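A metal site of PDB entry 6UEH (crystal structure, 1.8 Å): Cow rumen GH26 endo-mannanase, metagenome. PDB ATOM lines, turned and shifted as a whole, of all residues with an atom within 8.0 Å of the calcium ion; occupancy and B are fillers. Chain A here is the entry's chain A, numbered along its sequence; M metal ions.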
ATOM      1  N   ILE A  12      -1.819  21.578  -2.925  1.00  0.00           N
ATOM      2  CA  ILE A  12      -2.950  22.497  -2.970  1.00  0.00           C
ATOM      3  C   ILE A  12      -4.197  21.816  -3.500  1.00  0.00           C
ATOM      4  O   ILE A  12      -4.124  20.864  -4.282  1.00  0.00           O
ATOM      5  CB  ILE A  12      -2.664  23.704  -3.866  1.00  0.00           C
ATOM      6  CG1 ILE A  12      -2.188  23.227  -5.230  1.00  0.00           C
ATOM      7  CG2 ILE A  12      -1.627  24.592  -3.231  1.00  0.00           C
ATOM      8  CD1 ILE A  12      -2.311  24.279  -6.287  1.00  0.00           C
ATOM      9  N   GLU A  13      -5.354  22.309  -3.062  1.00  0.00           N
ATOM     10  CA  GLU A  13      -6.606  21.940  -3.693  1.00  0.00           C
ATOM     11  C   GLU A  13      -6.649  22.623  -5.054  1.00  0.00           C
ATOM     12  O   GLU A  13      -6.453  23.837  -5.141  1.00  0.00           O
ATOM     13  CB  GLU A  13      -7.809  22.347  -2.828  1.00  0.00           C
ATOM     14  CG  GLU A  13      -7.802  21.734  -1.437  1.00  0.00           C
ATOM     15  CD  GLU A  13      -8.106  20.236  -1.445  1.00  0.00           C
ATOM     16  OE1 GLU A  13      -8.598  19.741  -2.479  1.00  0.00           O
ATOM     17  OE2 GLU A  13      -7.853  19.569  -0.420  1.00  0.00           O
ATOM     18  N   ALA A  14      -6.883  21.867  -6.105  1.00  0.00           N
ATOM     19  CA  ALA A  14      -6.836  22.436  -7.451  1.00  0.00           C
ATOM     20  C   ALA A  14      -7.938  23.460  -7.653  1.00  0.00           C
ATOM     21  O   ALA A  14      -7.790  24.405  -8.426  1.00  0.00           O
ATOM     22  CB  ALA A  14      -6.922  21.347  -8.497  1.00  0.00           C
ATOM     23  N   GLU A  15      -9.046  23.289  -6.934  1.00  0.00           N
ATOM     24  CA  GLU A  15     -10.157  24.231  -7.017  1.00  0.00           C
ATOM     25  C   GLU A  15      -9.775  25.606  -6.469  1.00  0.00           C
ATOM     26  O   GLU A  15     -10.476  26.583  -6.701  1.00  0.00           O
ATOM     27  CB  GLU A  15     -11.395  23.696  -6.279  1.00  0.00           C
ATOM     28  CG  GLU A  15     -11.184  23.387  -4.794  1.00  0.00           C
ATOM     29  CD  GLU A  15     -10.781  21.939  -4.547  1.00  0.00           C
ATOM     30  OE1 GLU A  15     -10.220  21.309  -5.466  1.00  0.00           O
ATOM     31  OE2 GLU A  15     -11.028  21.426  -3.431  1.00  0.00           O
ATOM     32  N   ASP A  16      -8.648  25.672  -5.759  1.00  0.00           N
ATOM     33  CA  ASP A  16      -8.160  26.944  -5.224  1.00  0.00           C
ATOM     34  C   ASP A  16      -7.167  27.632  -6.172  1.00  0.00           C
ATOM     35  O   ASP A  16      -6.735  28.750  -5.903  1.00  0.00           O
ATOM     36  CB  ASP A  16      -7.515  26.735  -3.851  1.00  0.00           C
ATOM     37  CG  ASP A  16      -8.514  26.335  -2.788  1.00  0.00           C
ATOM     38  OD1 ASP A  16      -9.726  26.615  -2.968  1.00  0.00           O
ATOM     39  OD2 ASP A  16      -8.102  25.745  -1.773  1.00  0.00           O
ATOM     40  N   PRO A  23     -15.529  25.659  -6.969  1.00  0.00           N
ATOM     41  CA  PRO A  23     -15.276  24.213  -7.022  1.00  0.00           C
ATOM     42  C   PRO A  23     -16.383  23.439  -7.729  1.00  0.00           C
ATOM     43  O   PRO A  23     -17.564  23.767  -7.573  1.00  0.00           O
ATOM     44  CB  PRO A  23     -15.204  23.809  -5.537  1.00  0.00           C
ATOM     45  CG  PRO A  23     -14.883  25.077  -4.814  1.00  0.00           C
ATOM     46  CD  PRO A  23     -15.571  26.155  -5.582  1.00  0.00           C
ATOM     47  N   TRP A  24     -15.992  22.437  -8.503  1.00  0.00           N
ATOM     48  CA  TRP A  24     -16.944  21.520  -9.136  1.00  0.00           C
ATOM     49  C   TRP A  24     -17.152  20.298  -8.255  1.00  0.00           C
ATOM     50  O   TRP A  24     -16.258  19.919  -7.501  1.00  0.00           O
ATOM     51  CB  TRP A  24     -16.437  21.075 -10.512  1.00  0.00           C
ATOM     52  CG  TRP A  24     -16.263  22.184 -11.507  1.00  0.00           C
ATOM     53  CD1 TRP A  24     -15.295  23.150 -11.514  1.00  0.00           C
ATOM     54  CD2 TRP A  24     -17.083  22.428 -12.657  1.00  0.00           C
ATOM     55  NE1 TRP A  24     -15.474  23.983 -12.591  1.00  0.00           N
ATOM     56  CE2 TRP A  24     -16.562  23.564 -13.303  1.00  0.00           C
ATOM     57  CE3 TRP A  24     -18.207  21.799 -13.190  1.00  0.00           C
ATOM     58  CZ2 TRP A  24     -17.128  24.076 -14.474  1.00  0.00           C
ATOM     59  CZ3 TRP A  24     -18.771  22.319 -14.350  1.00  0.00           C
ATOM     60  CH2 TRP A  24     -18.235  23.448 -14.976  1.00  0.00           C
ATOM     61  N   MET A  35     -13.984   9.822  -3.739  1.00  0.00           N
ATOM     62  CA  MET A  35     -14.150  11.027  -2.936  1.00  0.00           C
ATOM     63  C   MET A  35     -13.052  12.050  -3.211  1.00  0.00           C
ATOM     64  O   MET A  35     -11.872  11.747  -3.078  1.00  0.00           O
ATOM     65  CB  MET A  35     -14.149  10.666  -1.447  1.00  0.00           C
ATOM     66  CG  MET A  35     -14.237  11.875  -0.516  1.00  0.00           C
ATOM     67  SD  MET A  35     -15.923  12.430  -0.248  1.00  0.00           S
ATOM     68  CE  MET A  35     -15.671  13.660   1.030  1.00  0.00           C
ATOM     69  N   TYR A  36     -13.451  13.264  -3.595  1.00  0.00           N
ATOM     70  CA  TYR A  36     -12.497  14.338  -3.769  1.00  0.00           C
ATOM     71  C   TYR A  36     -12.095  14.926  -2.421  1.00  0.00           C
ATOM     72  O   TYR A  36     -12.824  14.795  -1.427  1.00  0.00           O
ATOM     73  CB  TYR A  36     -13.056  15.442  -4.679  1.00  0.00           C
ATOM     74  CG  TYR A  36     -14.457  15.908  -4.325  1.00  0.00           C
ATOM     75  CD1 TYR A  36     -14.710  16.597  -3.147  1.00  0.00           C
ATOM     76  CD2 TYR A  36     -15.520  15.672  -5.194  1.00  0.00           C
ATOM     77  CE1 TYR A  36     -15.991  17.027  -2.830  1.00  0.00           C
ATOM     78  CE2 TYR A  36     -16.797  16.100  -4.886  1.00  0.00           C
ATOM     79  CZ  TYR A  36     -17.027  16.781  -3.707  1.00  0.00           C
ATOM     80  OH  TYR A  36     -18.298  17.202  -3.395  1.00  0.00           O
ATOM     81  N   SER A  37     -10.920  15.557  -2.381  1.00  0.00           N
ATOM     82  CA  SER A  37     -10.477  16.269  -1.197  1.00  0.00           C
ATOM     83  C   SER A  37     -11.048  17.681  -1.209  1.00  0.00           C
ATOM     84  O   SER A  37     -11.257  18.262  -2.279  1.00  0.00           O
ATOM     85  CB  SER A  37      -8.944  16.292  -1.123  1.00  0.00           C
ATOM     86  OG  SER A  37      -8.492  16.959   0.037  1.00  0.00           O
ATOM     87  N   GLY A  38     -11.303  18.242  -0.038  1.00  0.00           N
ATOM     88  CA  GLY A  38     -11.823  19.595   0.051  1.00  0.00           C
ATOM     89  C   GLY A  38     -13.261  19.719  -0.434  1.00  0.00           C
ATOM     90  O   GLY A  38     -14.044  18.782  -0.305  1.00  0.00           O
ATOM     91  N   LYS A  39     -13.592  20.883  -0.990  1.00  0.00           N
ATOM     92  CA  LYS A  39     -14.977  21.177  -1.360  1.00  0.00           C
ATOM     93  C   LYS A  39     -15.348  20.641  -2.733  1.00  0.00           C
ATOM     94  O   LYS A  39     -16.520  20.608  -3.099  1.00  0.00           O
ATOM     95  CB  LYS A  39     -15.222  22.687  -1.300  1.00  0.00           C
ATOM     96  CG  LYS A  39     -15.100  23.276   0.100  1.00  0.00           C
ATOM     97  CD  LYS A  39     -15.367  24.775   0.093  1.00  0.00           C
ATOM     98  CE  LYS A  39     -15.328  25.345   1.499  1.00  0.00           C
ATOM     99  NZ  LYS A  39     -15.560  26.814   1.514  1.00  0.00           N
ATOM    100  N   GLY A  40     -14.344  20.225  -3.505  1.00  0.00           N
ATOM    101  CA  GLY A  40     -14.607  19.691  -4.825  1.00  0.00           C
ATOM    102  C   GLY A  40     -13.350  19.545  -5.664  1.00  0.00           C
ATOM    103  O   GLY A  40     -12.317  19.080  -5.178  1.00  0.00           O
ATOM    104  N   PHE A  41     -13.432  19.933  -6.927  1.00  0.00           N
ATOM    105  CA  PHE A  41     -12.281  19.857  -7.818  1.00  0.00           C
ATOM    106  C   PHE A  41     -12.315  20.942  -8.891  1.00  0.00           C
ATOM    107  O   PHE A  41     -13.324  21.632  -9.058  1.00  0.00           O
ATOM    108  CB  PHE A  41     -12.199  18.473  -8.470  1.00  0.00           C
ATOM    109  CG  PHE A  41     -13.409  18.105  -9.294  1.00  0.00           C
ATOM    110  CD1 PHE A  41     -13.460  18.405 -10.642  1.00  0.00           C
ATOM    111  CD2 PHE A  41     -14.484  17.448  -8.718  1.00  0.00           C
ATOM    112  CE1 PHE A  41     -14.565  18.068 -11.406  1.00  0.00           C
ATOM    113  CE2 PHE A  41     -15.594  17.098  -9.472  1.00  0.00           C
ATOM    114  CZ  PHE A  41     -15.631  17.411 -10.815  1.00  0.00           C
ATOM    115  N   ALA A  42     -11.204  21.077  -9.604  1.00  0.00           N
ATOM    116  CA  ALA A  42     -11.130  21.983 -10.734  1.00  0.00           C
ATOM    117  C   ALA A  42     -11.428  21.234 -12.021  1.00  0.00           C
ATOM    118  O   ALA A  42     -10.878  20.164 -12.268  1.00  0.00           O
ATOM    119  CB  ALA A  42      -9.763  22.650 -10.806  1.00  0.00           C
ATOM    120  N   LYS A  66      -3.875  14.490  -8.259  1.00  0.00           N
ATOM    121  CA  LYS A  66      -5.009  13.581  -8.185  1.00  0.00           C
ATOM    122  C   LYS A  66      -5.998  13.998  -9.251  1.00  0.00           C
ATOM    123  O   LYS A  66      -6.658  15.038  -9.133  1.00  0.00           O
ATOM    124  CB  LYS A  66      -5.652  13.612  -6.799  1.00  0.00           C
ATOM    125  CG  LYS A  66      -6.685  12.513  -6.582  1.00  0.00           C
ATOM    126  CD  LYS A  66      -6.017  11.211  -6.188  1.00  0.00           C
ATOM    127  CE  LYS A  66      -5.343  11.348  -4.824  1.00  0.00           C
ATOM    128  NZ  LYS A  66      -4.679  10.084  -4.404  1.00  0.00           N
ATOM    129  N   TRP A  97     -10.811   9.053  -9.110  1.00  0.00           N
ATOM    130  CA  TRP A  97      -9.648   9.862  -8.762  1.00  0.00           C
ATOM    131  C   TRP A  97      -8.376   9.028  -8.738  1.00  0.00           C
ATOM    132  O   TRP A  97      -8.300   8.005  -8.057  1.00  0.00           O
ATOM    133  CB  TRP A  97      -9.846  10.568  -7.425  1.00  0.00           C
ATOM    134  CG  TRP A  97     -10.949  11.571  -7.456  1.00  0.00           C
ATOM    135  CD1 TRP A  97     -12.122  11.533  -6.752  1.00  0.00           C
ATOM    136  CD2 TRP A  97     -10.996  12.759  -8.257  1.00  0.00           C
ATOM    137  NE1 TRP A  97     -12.892  12.624  -7.056  1.00  0.00           N
ATOM    138  CE2 TRP A  97     -12.233  13.395  -7.978  1.00  0.00           C
ATOM    139  CE3 TRP A  97     -10.126  13.354  -9.173  1.00  0.00           C
ATOM    140  CZ2 TRP A  97     -12.598  14.586  -8.589  1.00  0.00           C
ATOM    141  CZ3 TRP A  97     -10.502  14.540  -9.778  1.00  0.00           C
ATOM    142  CH2 TRP A  97     -11.723  15.140  -9.487  1.00  0.00           C
ATOM    143  N   PHE A 125      -9.100  17.950 -11.863  1.00  0.00           N
ATOM    144  CA  PHE A 125      -7.985  18.030 -10.925  1.00  0.00           C
ATOM    145  C   PHE A 125      -8.503  18.245  -9.501  1.00  0.00           C
ATOM    146  O   PHE A 125      -9.128  19.255  -9.205  1.00  0.00           O
ATOM    147  CB  PHE A 125      -7.028  19.156 -11.318  1.00  0.00           C
ATOM    148  CG  PHE A 125      -6.379  18.951 -12.655  1.00  0.00           C
ATOM    149  CD1 PHE A 125      -7.049  19.258 -13.829  1.00  0.00           C
ATOM    150  CD2 PHE A 125      -5.083  18.447 -12.741  1.00  0.00           C
ATOM    151  CE1 PHE A 125      -6.441  19.066 -15.053  1.00  0.00           C
ATOM    152  CE2 PHE A 125      -4.480  18.263 -13.969  1.00  0.00           C
ATOM    153  CZ  PHE A 125      -5.159  18.572 -15.125  1.00  0.00           C
ATOM    154  N   ASP A 126      -8.241  17.271  -8.633  1.00  0.00           N
ATOM    155  CA  ASP A 126      -8.672  17.348  -7.238  1.00  0.00           C
ATOM    156  C   ASP A 126      -7.637  18.083  -6.393  1.00  0.00           C
ATOM    157  O   ASP A 126      -7.948  19.081  -5.747  1.00  0.00           O
ATOM    158  CB  ASP A 126      -8.904  15.944  -6.671  1.00  0.00           C
ATOM    159  CG  ASP A 126      -9.393  15.958  -5.229  1.00  0.00           C
ATOM    160  OD1 ASP A 126      -9.950  16.994  -4.800  1.00  0.00           O
ATOM    161  OD2 ASP A 126      -9.221  14.934  -4.534  1.00  0.00           O
ATOM    162  N   THR A 127      -6.413  17.565  -6.400  1.00  0.00           N
ATOM    163  CA  THR A 127      -5.289  18.213  -5.724  1.00  0.00           C
ATOM    164  C   THR A 127      -4.051  18.179  -6.610  1.00  0.00           C
ATOM    165  O   THR A 127      -3.978  17.392  -7.549  1.00  0.00           O
ATOM    166  CB  THR A 127      -4.952  17.516  -4.383  1.00  0.00           C
ATOM    167  OG1 THR A 127      -4.619  16.147  -4.620  1.00  0.00           O
ATOM    168  CG2 THR A 127      -6.120  17.594  -3.411  1.00  0.00           C
ATOM    169  N   ILE A 128      -3.094  19.038  -6.305  1.00  0.00           N
ATOM    170  CA  ILE A 128      -1.817  19.053  -6.998  1.00  0.00           C
ATOM    171  C   ILE A 128      -0.696  19.049  -5.967  1.00  0.00           C
ATOM    172  O   ILE A 128      -0.778  19.758  -4.954  1.00  0.00           O
ATOM    173  CB  ILE A 128      -1.683  20.293  -7.918  1.00  0.00           C
ATOM    174  CG1 ILE A 128      -2.856  20.349  -8.903  1.00  0.00           C
ATOM    175  CG2 ILE A 128      -0.352  20.271  -8.658  1.00  0.00           C
ATOM    176  CD1 ILE A 128      -3.051  21.707  -9.553  1.00  0.00           C
HETATM  177 CA    CA M   1     -10.142  19.199  -4.167  1.00  0.00          CA
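The backbone NH (N) of Ala 14 lies close to the backbone carbonyl oxygen (O) of Asp 126 (3.0 Å). The backbone NH (N) of Asp 126 is in hydrogen-bond range of the backbone carbonyl oxygen (O) of Lys 66 (2.8 Å).
Within 4 Å of the calcium ion: Glu 13, Glu 15, Ser 37, Gly 40 and Asp 126.
The calcium ion is bound by the side-chain carboxylate (OD1) of Asp 126 (2.3 Å), the side-chain carboxylate (OE1) of Glu 13 (2.4 Å), the backbone carbonyl oxygen (O) of Ser 37 (2.4 Å), the backbone carbonyl oxygen (O) of Gly 40 (2.4 Å), the side-chain carboxylate (OE1) of Glu 15 (2.5 Å), the side-chain carboxylate (OE2) of Glu 15 (2.5 Å) and the backbone carbonyl oxygen (O) of Asp 126 (2.7 Å). The calcium ion has seven donor atoms within binding distance.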
